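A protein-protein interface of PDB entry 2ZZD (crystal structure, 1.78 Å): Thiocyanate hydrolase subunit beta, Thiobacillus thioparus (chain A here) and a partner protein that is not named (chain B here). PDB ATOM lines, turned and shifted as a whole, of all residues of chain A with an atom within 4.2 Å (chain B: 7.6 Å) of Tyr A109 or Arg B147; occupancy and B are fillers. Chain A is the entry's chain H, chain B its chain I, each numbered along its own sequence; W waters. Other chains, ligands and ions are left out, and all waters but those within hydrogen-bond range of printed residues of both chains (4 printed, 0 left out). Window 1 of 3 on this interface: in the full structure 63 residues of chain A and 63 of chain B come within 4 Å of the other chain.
Of the 10 printed residues of chain A, 8 touch a printed residue of chain B. Hydrophobic or aromatic side chains of chain A within 4 Å of the printed part of chain B: Trp A68, Phe A73, Pro A107, Tyr A108, Tyr A109, Trp A112 and Leu A113. Of the 22 printed residues of chain B, 6 touch a printed residue of chain A. Hydrophobic or aromatic side chains of chain B within 4 Å of the printed part of chain A: Phe B27 and Val B56. Among the printed residues, 12 pairs touch across the chains. Among the printed residues, no Asp or Glu carboxylate lies within 4 Å of a Lys or Arg side-chain nitrogen of the other chain.
Arg B147 touches just these residues of chain A: Tyr A108 (3.5 Å) and Tyr A109 (3.5 Å). Of the printed residues of chain B, Tyr A108 touches Ser B132 and Arg B147. Printed residues of chain B within 4 Å of Pro A107: Phe B27 (3.8 Å). Printed residues of chain A within 4 Å of Phe B27: Trp A68, Pro A107, Gly A110 and Leu A113. Of the printed residues of chain A, Ser B132 touches Tyr A108. Printed residues of chain A within 4 Å of Gln B141: Phe A73 (3.5 Å) and Tyr A109 (3.6 Å). The nearest residue of chain B that does not touch Tyr A109 is Arg B136 (5.1 Å). The nearest printed residue of chain B that does not touch Leu A113 is Arg B147 (11.2 Å).
The guanidinium group of Arg B136 sits at hydrogen-bond distance from the side-chain amide oxygen of Gln B141 (3.1 Å). The side-chain hydroxyl (OG) of Ser B142 is in hydrogen-bond range of the guanidinium group (NE) of Arg B147 (2.9 Å). OE1 of Glu B144 is in salt-bridge range of NH1 of Arg B147.
OG of Ser B132 sits at hydrogen-bond distance from OH of Tyr A108.
CB of Phe B27 touches CE2 of Trp A68 (3.5 Å). CE2 of Phe A73 touches CG2 of Val B56 (3.8 Å). CZ of Phe A73 touches NE of Arg B136, 3.6 Å away. Gln B141 touches Phe A73. Tyr A108 touches Arg B147. OH of Tyr A109 touches NE2 of Gln B141 (3.6 Å). Tyr A109 touches Arg B147 (CE2 to NH1, 3.5 Å). Phe B27 touches Gly A110 (CE1 to CA, 3.7 Å). Arg B136 touches Trp A112 (NH2 to CH2, 3.9 Å). Phe B27 touches Leu A113.
Water W1 bridges OH of Tyr A109 and NE2 of Gln B141. Water W2 lies within hydrogen-bond range of the side-chain hydroxyl of Tyr A109, the side-chain hydroxyl of Tyr A108, the guanidinium group of Arg B136 and the side-chain amide oxygen of Gln B141. Water W3 lies within hydrogen-bond range of OE1 of Glu A69 and NH1 of Arg B147. Water W4 bridges the side-chain hydroxyl of Ser B132 (3.0 Å) and the indole nitrogen of Trp A112 (3.3 Å).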
ATOM      1  N   TRP A  68       2.615   0.653   8.340  1.00  0.00           N
ATOM      2  CA  TRP A  68       2.715  -0.801   8.363  1.00  0.00           C
ATOM      3  C   TRP A  68       3.036  -1.353   9.747  1.00  0.00           C
ATOM      4  O   TRP A  68       2.680  -2.488  10.052  1.00  0.00           O
ATOM      5  CB  TRP A  68       3.733  -1.327   7.326  1.00  0.00           C
ATOM      6  CG  TRP A  68       5.198  -1.149   7.642  1.00  0.00           C
ATOM      7  CD1 TRP A  68       6.026  -0.159   7.185  1.00  0.00           C
ATOM      8  CD2 TRP A  68       6.022  -2.030   8.422  1.00  0.00           C
ATOM      9  NE1 TRP A  68       7.313  -0.377   7.625  1.00  0.00           N
ATOM     10  CE2 TRP A  68       7.337  -1.514   8.388  1.00  0.00           C
ATOM     11  CE3 TRP A  68       5.774  -3.206   9.144  1.00  0.00           C
ATOM     12  CZ2 TRP A  68       8.406  -2.138   9.050  1.00  0.00           C
ATOM     13  CZ3 TRP A  68       6.840  -3.830   9.805  1.00  0.00           C
ATOM     14  CH2 TRP A  68       8.140  -3.290   9.752  1.00  0.00           C
ATOM     15  N   GLU A  69       3.687  -0.556  10.591  1.00  0.00           N
ATOM     16  CA  GLU A  69       4.010  -1.011  11.942  1.00  0.00           C
ATOM     17  C   GLU A  69       2.739  -1.033  12.790  1.00  0.00           C
ATOM     18  O   GLU A  69       2.517  -1.958  13.574  1.00  0.00           O
ATOM     19  CB  GLU A  69       5.053  -0.095  12.593  1.00  0.00           C
ATOM     20  CG  GLU A  69       6.445  -0.230  11.979  1.00  0.00           C
ATOM     21  CD  GLU A  69       7.451   0.738  12.578  1.00  0.00           C
ATOM     22  OE1 GLU A  69       7.054   1.877  12.902  1.00  0.00           O
ATOM     23  OE2 GLU A  69       8.638   0.367  12.714  1.00  0.00           O
ATOM     24  N   PHE A  73       1.180  -4.437  14.420  1.00  0.00           N
ATOM     25  CA  PHE A  73       0.872  -4.583  15.834  1.00  0.00           C
ATOM     26  C   PHE A  73      -0.569  -5.064  16.012  1.00  0.00           C
ATOM     27  O   PHE A  73      -0.833  -6.005  16.764  1.00  0.00           O
ATOM     28  CB  PHE A  73       1.070  -3.256  16.573  1.00  0.00           C
ATOM     29  CG  PHE A  73       0.799  -3.350  18.044  1.00  0.00           C
ATOM     30  CD1 PHE A  73       1.610  -4.130  18.865  1.00  0.00           C
ATOM     31  CD2 PHE A  73      -0.302  -2.703  18.603  1.00  0.00           C
ATOM     32  CE1 PHE A  73       1.326  -4.272  20.224  1.00  0.00           C
ATOM     33  CE2 PHE A  73      -0.595  -2.838  19.961  1.00  0.00           C
ATOM     34  CZ  PHE A  73       0.222  -3.626  20.772  1.00  0.00           C
ATOM     35  N   PRO A 107      14.743  -4.902  11.748  1.00  0.00           N
ATOM     36  CA  PRO A 107      14.037  -3.983  12.644  1.00  0.00           C
ATOM     37  C   PRO A 107      13.073  -4.690  13.588  1.00  0.00           C
ATOM     38  O   PRO A 107      12.561  -5.770  13.290  1.00  0.00           O
ATOM     39  CB  PRO A 107      13.274  -3.059  11.687  1.00  0.00           C
ATOM     40  CG  PRO A 107      13.945  -3.269  10.339  1.00  0.00           C
ATOM     41  CD  PRO A 107      14.278  -4.728  10.363  1.00  0.00           C
ATOM     42  N   TYR A 108      12.836  -4.039  14.720  1.00  0.00           N
ATOM     43  CA  TYR A 108      11.924  -4.494  15.757  1.00  0.00           C
ATOM     44  C   TYR A 108      10.602  -4.992  15.147  1.00  0.00           C
ATOM     45  O   TYR A 108      10.256  -6.168  15.273  1.00  0.00           O
ATOM     46  CB  TYR A 108      11.694  -3.313  16.710  1.00  0.00           C
ATOM     47  CG  TYR A 108      10.618  -3.463  17.762  1.00  0.00           C
ATOM     48  CD1 TYR A 108      10.916  -3.955  19.035  1.00  0.00           C
ATOM     49  CD2 TYR A 108       9.324  -3.014  17.514  1.00  0.00           C
ATOM     50  CE1 TYR A 108       9.950  -3.976  20.042  1.00  0.00           C
ATOM     51  CE2 TYR A 108       8.347  -3.041  18.505  1.00  0.00           C
ATOM     52  CZ  TYR A 108       8.668  -3.516  19.769  1.00  0.00           C
ATOM     53  OH  TYR A 108       7.713  -3.496  20.760  1.00  0.00           O
ATOM     54  N   TYR A 109       9.868  -4.110  14.474  1.00  0.00           N
ATOM     55  CA  TYR A 109       8.600  -4.520  13.881  1.00  0.00           C
ATOM     56  C   TYR A 109       8.756  -5.442  12.675  1.00  0.00           C
ATOM     57  O   TYR A 109       7.796  -6.092  12.257  1.00  0.00           O
ATOM     58  CB  TYR A 109       7.749  -3.301  13.528  1.00  0.00           C
ATOM     59  CG  TYR A 109       6.808  -2.922  14.651  1.00  0.00           C
ATOM     60  CD1 TYR A 109       5.887  -3.849  15.152  1.00  0.00           C
ATOM     61  CD2 TYR A 109       6.844  -1.653  15.228  1.00  0.00           C
ATOM     62  CE1 TYR A 109       5.030  -3.521  16.199  1.00  0.00           C
ATOM     63  CE2 TYR A 109       5.985  -1.318  16.281  1.00  0.00           C
ATOM     64  CZ  TYR A 109       5.082  -2.256  16.759  1.00  0.00           C
ATOM     65  OH  TYR A 109       4.232  -1.928  17.795  1.00  0.00           O
ATOM     66  N   GLY A 110       9.960  -5.502  12.114  1.00  0.00           N
ATOM     67  CA  GLY A 110      10.189  -6.404  11.000  1.00  0.00           C
ATOM     68  C   GLY A 110      10.066  -7.821  11.547  1.00  0.00           C
ATOM     69  O   GLY A 110       9.525  -8.724  10.900  1.00  0.00           O
ATOM     70  N   ARG A 111      10.572  -8.019  12.761  1.00  0.00           N
ATOM     71  CA  ARG A 111      10.502  -9.331  13.397  1.00  0.00           C
ATOM     72  C   ARG A 111       9.059  -9.653  13.802  1.00  0.00           C
ATOM     73  O   ARG A 111       8.629 -10.807  13.715  1.00  0.00           O
ATOM     74  CB  ARG A 111      11.433  -9.385  14.612  1.00  0.00           C
ATOM     75  CG  ARG A 111      12.904  -9.264  14.228  1.00  0.00           C
ATOM     76  CD  ARG A 111      13.849  -9.413  15.422  1.00  0.00           C
ATOM     77  NE  ARG A 111      13.669  -8.361  16.420  1.00  0.00           N
ATOM     78  CZ  ARG A 111      12.954  -8.498  17.533  1.00  0.00           C
ATOM     79  NH1 ARG A 111      12.343  -9.646  17.802  1.00  0.00           N
ATOM     80  NH2 ARG A 111      12.857  -7.486  18.387  1.00  0.00           N
ATOM     81  N   TRP A 112       8.315  -8.644  14.251  1.00  0.00           N
ATOM     82  CA  TRP A 112       6.919  -8.859  14.627  1.00  0.00           C
ATOM     83  C   TRP A 112       6.151  -9.357  13.399  1.00  0.00           C
ATOM     84  O   TRP A 112       5.393 -10.321  13.477  1.00  0.00           O
ATOM     85  CB  TRP A 112       6.255  -7.561  15.102  1.00  0.00           C
ATOM     86  CG  TRP A 112       6.501  -7.178  16.532  1.00  0.00           C
ATOM     87  CD1 TRP A 112       7.675  -6.745  17.079  1.00  0.00           C
ATOM     88  CD2 TRP A 112       5.520  -7.104  17.578  1.00  0.00           C
ATOM     89  NE1 TRP A 112       7.483  -6.394  18.400  1.00  0.00           N
ATOM     90  CE2 TRP A 112       6.171  -6.605  18.730  1.00  0.00           C
ATOM     91  CE3 TRP A 112       4.151  -7.406  17.653  1.00  0.00           C
ATOM     92  CZ2 TRP A 112       5.498  -6.400  19.947  1.00  0.00           C
ATOM     93  CZ3 TRP A 112       3.482  -7.201  18.862  1.00  0.00           C
ATOM     94  CH2 TRP A 112       4.159  -6.702  19.991  1.00  0.00           C
ATOM     95  N   LEU A 113       6.353  -8.681  12.270  1.00  0.00           N
ATOM     96  CA  LEU A 113       5.667  -9.029  11.026  1.00  0.00           C
ATOM     97  C   LEU A 113       6.054 -10.400  10.478  1.00  0.00           C
ATOM     98  O   LEU A 113       5.185 -11.191  10.101  1.00  0.00           O
ATOM     99  CB  LEU A 113       5.924  -7.953   9.966  1.00  0.00           C
ATOM    100  CG  LEU A 113       5.315  -8.212   8.587  1.00  0.00           C
ATOM    101  CD1 LEU A 113       3.807  -8.431   8.706  1.00  0.00           C
ATOM    102  CD2 LEU A 113       5.611  -7.030   7.674  1.00  0.00           C
ATOM    103  N   PHE B  27       8.350  -4.664   3.647  1.00  0.00           N
ATOM    104  CA  PHE B  27       7.550  -4.789   4.864  1.00  0.00           C
ATOM    105  C   PHE B  27       6.083  -4.475   4.589  1.00  0.00           C
ATOM    106  O   PHE B  27       5.192  -5.122   5.136  1.00  0.00           O
ATOM    107  CB  PHE B  27       8.067  -3.848   5.952  1.00  0.00           C
ATOM    108  CG  PHE B  27       9.471  -4.144   6.389  1.00  0.00           C
ATOM    109  CD1 PHE B  27       9.762  -5.289   7.133  1.00  0.00           C
ATOM    110  CD2 PHE B  27      10.508  -3.279   6.048  1.00  0.00           C
ATOM    111  CE1 PHE B  27      11.077  -5.570   7.536  1.00  0.00           C
ATOM    112  CE2 PHE B  27      11.819  -3.548   6.442  1.00  0.00           C
ATOM    113  CZ  PHE B  27      12.107  -4.695   7.186  1.00  0.00           C
ATOM    114  N   VAL B  56      -5.978   1.209  20.035  1.00  0.00           N
ATOM    115  CA  VAL B  56      -4.616   1.692  20.227  1.00  0.00           C
ATOM    116  C   VAL B  56      -4.559   3.206  20.039  1.00  0.00           C
ATOM    117  O   VAL B  56      -3.829   3.897  20.749  1.00  0.00           O
ATOM    118  CB  VAL B  56      -3.628   1.008  19.247  1.00  0.00           C
ATOM    119  CG1 VAL B  56      -2.253   1.652  19.347  1.00  0.00           C
ATOM    120  CG2 VAL B  56      -3.524  -0.479  19.573  1.00  0.00           C
ATOM    121  N   VAL B 127      12.299  -1.108  32.598  1.00  0.00           N
ATOM    122  CA  VAL B 127      12.802  -1.640  31.335  1.00  0.00           C
ATOM    123  C   VAL B 127      12.292  -3.071  31.172  1.00  0.00           C
ATOM    124  O   VAL B 127      11.818  -3.679  32.127  1.00  0.00           O
ATOM    125  CB  VAL B 127      14.358  -1.680  31.322  1.00  0.00           C
ATOM    126  CG1 VAL B 127      14.868  -2.635  32.399  1.00  0.00           C
ATOM    127  CG2 VAL B 127      14.871  -2.126  29.956  1.00  0.00           C
ATOM    128  N   CYS B 128      12.363  -3.586  29.949  1.00  0.00           N
ATOM    129  CA  CYS B 128      12.000  -4.971  29.661  1.00  0.00           C
ATOM    130  C   CYS B 128      13.241  -5.449  28.923  1.00  0.00           C
ATOM    131  O   CYS B 128      13.352  -5.249  27.715  1.00  0.00           O
ATOM    132  CB  CYS B 128      10.791  -5.068  28.732  1.00  0.00           C
ATOM    133  SG  CYS B 128      10.431  -6.783  28.234  1.00  0.00           S
ATOM    134  N   THR B 129      14.186  -6.055  29.639  1.00  0.00           N
ATOM    135  CA  THR B 129      15.413  -6.483  28.984  1.00  0.00           C
ATOM    136  C   THR B 129      15.188  -7.538  27.912  1.00  0.00           C
ATOM    137  O   THR B 129      15.953  -7.613  26.954  1.00  0.00           O
ATOM    138  CB  THR B 129      16.456  -7.030  29.990  1.00  0.00           C
ATOM    139  OG1 THR B 129      15.934  -8.187  30.655  1.00  0.00           O
ATOM    140  CG2 THR B 129      16.819  -5.964  31.020  1.00  0.00           C
ATOM    141  N   CSD B 131      12.563  -7.717  25.905  1.00  0.00           N
ATOM    142  CA  CSD B 131      11.879  -7.142  24.756  1.00  0.00           C
ATOM    143  CB  CSD B 131      10.795  -8.057  24.180  1.00  0.00           C
ATOM    144  SG  CSD B 131       9.549  -8.553  25.426  1.00  0.00           S
ATOM    145  C   CSD B 131      11.439  -5.679  24.782  1.00  0.00           C
ATOM    146  O   CSD B 131      12.211  -4.786  24.438  1.00  0.00           O
ATOM    147  OD1 CSD B 131      10.117  -9.555  26.278  1.00  0.00           O
ATOM    148  OD2 CSD B 131       8.362  -9.127  24.708  1.00  0.00           O
ATOM    149  N   SER B 132      10.196  -5.430  25.184  1.00  0.00           N
ATOM    150  CA  SER B 132       9.701  -4.059  25.225  1.00  0.00           C
ATOM    151  C   SER B 132       8.455  -3.923  26.078  1.00  0.00           C
ATOM    152  O   SER B 132       7.752  -2.909  26.019  1.00  0.00           O
ATOM    153  CB  SER B 132       9.410  -3.563  23.809  1.00  0.00           C
ATOM    154  OG  SER B 132       8.501  -4.429  23.145  1.00  0.00           O
ATOM    155  N   CSD B 133       8.181  -4.958  26.863  1.00  0.00           N
ATOM    156  CA  CSD B 133       7.038  -4.956  27.755  1.00  0.00           C
ATOM    157  CB  CSD B 133       7.001  -6.182  28.638  1.00  0.00           C
ATOM    158  SG  CSD B 133       7.379  -7.643  27.609  1.00  0.00           S
ATOM    159  C   CSD B 133       6.776  -3.608  28.399  1.00  0.00           C
ATOM    160  O   CSD B 133       7.651  -3.040  29.049  1.00  0.00           O
ATOM    161  OD1 CSD B 133       6.288  -7.875  26.701  1.00  0.00           O
ATOM    162  OD2 CSD B 133       7.619  -8.847  28.461  1.00  0.00           O
ATOM    163  N   ARG B 136       0.942  -0.585  28.156  1.00  0.00           N
ATOM    164  CA  ARG B 136       0.184   0.075  27.095  1.00  0.00           C
ATOM    165  C   ARG B 136      -1.236   0.564  27.432  1.00  0.00           C
ATOM    166  O   ARG B 136      -1.589   1.697  27.111  1.00  0.00           O
ATOM    167  CB  ARG B 136       0.122  -0.825  25.851  1.00  0.00           C
ATOM    168  CG  ARG B 136       1.491  -1.173  25.227  1.00  0.00           C
ATOM    169  CD  ARG B 136       1.281  -1.821  23.855  1.00  0.00           C
ATOM    170  NE  ARG B 136       2.513  -2.243  23.183  1.00  0.00           N
ATOM    171  CZ  ARG B 136       3.053  -3.454  23.280  1.00  0.00           C
ATOM    172  NH1 ARG B 136       2.484  -4.384  24.034  1.00  0.00           N
ATOM    173  NH2 ARG B 136       4.146  -3.753  22.583  1.00  0.00           N
ATOM    174  N   GLY B 140       0.104   3.992  26.763  1.00  0.00           N
ATOM    175  CA  GLY B 140       0.257   4.170  25.324  1.00  0.00           C
ATOM    176  C   GLY B 140       1.370   3.289  24.767  1.00  0.00           C
ATOM    177  O   GLY B 140       1.772   2.340  25.432  1.00  0.00           O
ATOM    178  N   GLN B 141       1.865   3.578  23.559  1.00  0.00           N
ATOM    179  CA  GLN B 141       2.943   2.768  22.968  1.00  0.00           C
ATOM    180  C   GLN B 141       4.305   3.145  23.535  1.00  0.00           C
ATOM    181  O   GLN B 141       4.542   4.291  23.931  1.00  0.00           O
ATOM    182  CB  GLN B 141       3.010   2.919  21.440  1.00  0.00           C
ATOM    183  CG  GLN B 141       2.208   1.899  20.632  1.00  0.00           C
ATOM    184  CD  GLN B 141       2.664   0.457  20.827  1.00  0.00           C
ATOM    185  OE1 GLN B 141       3.598   0.169  21.586  1.00  0.00           O
ATOM    186  NE2 GLN B 141       1.992  -0.463  20.145  1.00  0.00           N
ATOM    187  N   SER B 142       5.200   2.166  23.549  1.00  0.00           N
ATOM    188  CA  SER B 142       6.551   2.351  24.060  1.00  0.00           C
ATOM    189  C   SER B 142       7.399   3.211  23.124  1.00  0.00           C
ATOM    190  O   SER B 142       7.186   3.216  21.912  1.00  0.00           O
ATOM    191  CB  SER B 142       7.219   0.985  24.243  1.00  0.00           C
ATOM    192  OG  SER B 142       7.223   0.253  23.023  1.00  0.00           O
ATOM    193  N   PRO B 143       8.362   3.964  23.686  1.00  0.00           N
ATOM    194  CA  PRO B 143       9.257   4.831  22.909  1.00  0.00           C
ATOM    195  C   PRO B 143      10.212   3.951  22.113  1.00  0.00           C
ATOM    196  O   PRO B 143      10.502   2.829  22.521  1.00  0.00           O
ATOM    197  CB  PRO B 143      10.015   5.613  23.979  1.00  0.00           C
ATOM    198  CG  PRO B 143       9.117   5.560  25.185  1.00  0.00           C
ATOM    199  CD  PRO B 143       8.571   4.157  25.131  1.00  0.00           C
ATOM    200  N   GLU B 144      10.711   4.461  20.996  1.00  0.00           N
ATOM    201  CA  GLU B 144      11.644   3.697  20.179  1.00  0.00           C
ATOM    202  C   GLU B 144      12.873   3.287  21.002  1.00  0.00           C
ATOM    203  O   GLU B 144      13.289   2.130  20.963  1.00  0.00           O
ATOM    204  CB  GLU B 144      12.084   4.525  18.963  1.00  0.00           C
ATOM    205  CG  GLU B 144      13.052   3.814  18.016  1.00  0.00           C
ATOM    206  CD  GLU B 144      12.380   2.782  17.127  1.00  0.00           C
ATOM    207  OE1 GLU B 144      11.152   2.579  17.256  1.00  0.00           O
ATOM    208  OE2 GLU B 144      13.090   2.164  16.304  1.00  0.00           O
ATOM    209  N   TRP B 145      13.439   4.224  21.763  1.00  0.00           N
ATOM    210  CA  TRP B 145      14.629   3.923  22.562  1.00  0.00           C
ATOM    211  C   TRP B 145      14.417   2.871  23.646  1.00  0.00           C
ATOM    212  O   TRP B 145      15.342   2.133  23.986  1.00  0.00           O
ATOM    213  CB  TRP B 145      15.214   5.198  23.190  1.00  0.00           C
ATOM    214  CG  TRP B 145      14.231   6.074  23.924  1.00  0.00           C
ATOM    215  CD1 TRP B 145      13.576   7.170  23.432  1.00  0.00           C
ATOM    216  CD2 TRP B 145      13.804   5.929  25.283  1.00  0.00           C
ATOM    217  NE1 TRP B 145      12.768   7.714  24.403  1.00  0.00           N
ATOM    218  CE2 TRP B 145      12.884   6.970  25.548  1.00  0.00           C
ATOM    219  CE3 TRP B 145      14.105   5.014  26.304  1.00  0.00           C
ATOM    220  CZ2 TRP B 145      12.265   7.126  26.796  1.00  0.00           C
ATOM    221  CZ3 TRP B 145      13.491   5.170  27.545  1.00  0.00           C
ATOM    222  CH2 TRP B 145      12.578   6.218  27.778  1.00  0.00           C
ATOM    223  N   TYR B 146      13.200   2.803  24.181  1.00  0.00           N
ATOM    224  CA  TYR B 146      12.854   1.837  25.221  1.00  0.00           C
ATOM    225  C   TYR B 146      12.984   0.414  24.669  1.00  0.00           C
ATOM    226  O   TYR B 146      13.297  -0.523  25.401  1.00  0.00           O
ATOM    227  CB  TYR B 146      11.413   2.084  25.677  1.00  0.00           C
ATOM    228  CG  TYR B 146      10.930   1.200  26.804  1.00  0.00           C
ATOM    229  CD1 TYR B 146      11.170   1.536  28.135  1.00  0.00           C
ATOM    230  CD2 TYR B 146      10.216   0.031  26.538  1.00  0.00           C
ATOM    231  CE1 TYR B 146      10.700   0.734  29.177  1.00  0.00           C
ATOM    232  CE2 TYR B 146       9.753  -0.782  27.567  1.00  0.00           C
ATOM    233  CZ  TYR B 146       9.995  -0.426  28.885  1.00  0.00           C
ATOM    234  OH  TYR B 146       9.532  -1.224  29.905  1.00  0.00           O
ATOM    235  N   ARG B 147      12.738   0.271  23.369  1.00  0.00           N
ATOM    236  CA  ARG B 147      12.808  -1.019  22.680  1.00  0.00           C
ATOM    237  C   ARG B 147      14.222  -1.362  22.215  1.00  0.00           C
ATOM    238  O   ARG B 147      14.476  -2.487  21.768  1.00  0.00           O
ATOM    239  CB  ARG B 147      11.931  -0.993  21.427  1.00  0.00           C
ATOM    240  CG  ARG B 147      10.514  -0.511  21.631  1.00  0.00           C
ATOM    241  CD  ARG B 147       9.854  -0.239  20.279  1.00  0.00           C
ATOM    242  NE  ARG B 147       8.515   0.309  20.452  1.00  0.00           N
ATOM    243  CZ  ARG B 147       7.726   0.708  19.459  1.00  0.00           C
ATOM    244  NH1 ARG B 147       8.133   0.622  18.199  1.00  0.00           N
ATOM    245  NH2 ARG B 147       6.529   1.213  19.731  1.00  0.00           N
ATOM    246  N   SER B 148      15.137  -0.402  22.301  1.00  0.00           N
ATOM    247  CA  SER B 148      16.491  -0.628  21.803  1.00  0.00           C
ATOM    248  C   SER B 148      17.334  -1.635  22.566  1.00  0.00           C
ATOM    249  O   SER B 148      17.270  -1.721  23.795  1.00  0.00           O
ATOM    250  CB  SER B 148      17.256   0.696  21.729  1.00  0.00           C
ATOM    251  OG  SER B 148      17.658   1.134  23.021  1.00  0.00           O
ATOM    252  N   PRO B 149      18.115  -2.444  21.833  1.00  0.00           N
ATOM    253  CA  PRO B 149      18.975  -3.431  22.483  1.00  0.00           C
ATOM    254  C   PRO B 149      19.883  -2.676  23.460  1.00  0.00           C
ATOM    255  O   PRO B 149      20.236  -3.181  24.525  1.00  0.00           O
ATOM    256  CB  PRO B 149      19.763  -4.013  21.317  1.00  0.00           C
ATOM    257  CG  PRO B 149      18.743  -4.028  20.219  1.00  0.00           C
ATOM    258  CD  PRO B 149      18.058  -2.674  20.377  1.00  0.00           C
ATOM    259  N   ASN B 150      20.241  -1.450  23.091  1.00  0.00           N
ATOM    260  CA  ASN B 150      21.124  -0.637  23.920  1.00  0.00           C
ATOM    261  C   ASN B 150      20.568  -0.370  25.321  1.00  0.00           C
ATOM    262  O   ASN B 150      21.234  -0.631  26.322  1.00  0.00           O
ATOM    263  CB  ASN B 150      21.426   0.685  23.215  1.00  0.00           C
ATOM    264  CG  ASN B 150      22.480   1.489  23.935  1.00  0.00           C
ATOM    265  OD1 ASN B 150      22.210   2.120  24.955  1.00  0.00           O
ATOM    266  ND2 ASN B 150      23.700   1.456  23.414  1.00  0.00           N
ATOM    267  N   TYR B 151      19.347   0.146  25.386  1.00  0.00           N
ATOM    268  CA  TYR B 151      18.696   0.449  26.661  1.00  0.00           C
ATOM    269  C   TYR B 151      18.486  -0.839  27.467  1.00  0.00           C
ATOM    270  O   TYR B 151      18.684  -0.875  28.686  1.00  0.00           O
ATOM    271  CB  TYR B 151      17.343   1.117  26.385  1.00  0.00           C
ATOM    272  CG  TYR B 151      16.559   1.546  27.607  1.00  0.00           C
ATOM    273  CD1 TYR B 151      16.927   2.676  28.342  1.00  0.00           C
ATOM    274  CD2 TYR B 151      15.407   0.857  27.987  1.00  0.00           C
ATOM    275  CE1 TYR B 151      16.155   3.114  29.425  1.00  0.00           C
ATOM    276  CE2 TYR B 151      14.629   1.287  29.066  1.00  0.00           C
ATOM    277  CZ  TYR B 151      15.007   2.414  29.778  1.00  0.00           C
ATOM    278  OH  TYR B 151      14.220   2.846  30.825  1.00  0.00           O
ATOM    279  N   ARG B 152      18.099  -1.899  26.766  1.00  0.00           N
ATOM    280  CA  ARG B 152      17.840  -3.190  27.388  1.00  0.00           C
ATOM    281  C   ARG B 152      19.105  -3.863  27.937  1.00  0.00           C
ATOM    282  O   ARG B 152      19.036  -4.640  28.891  1.00  0.00           O
ATOM    283  CB  ARG B 152      17.136  -4.095  26.380  1.00  0.00           C
ATOM    284  CG  ARG B 152      15.723  -3.611  26.029  1.00  0.00           C
ATOM    285  CD  ARG B 152      15.203  -4.323  24.792  1.00  0.00           C
ATOM    286  NE  ARG B 152      15.452  -5.754  24.888  1.00  0.00           N
ATOM    287  CZ  ARG B 152      15.759  -6.529  23.855  1.00  0.00           C
ATOM    288  NH1 ARG B 152      15.845  -6.009  22.636  1.00  0.00           N
ATOM    289  NH2 ARG B 152      16.014  -7.815  24.049  1.00  0.00           N
HETATM  290  O   HOH W   1       3.045   0.151  16.929  1.00  0.00           O
HETATM  291  O   HOH W   2       5.285  -2.175  20.308  1.00  0.00           O
HETATM  292  O   HOH W   3       7.023   2.176  15.770  1.00  0.00           O
HETATM  293  O   HOH W   4       8.886  -6.802  21.369  1.00  0.00           O
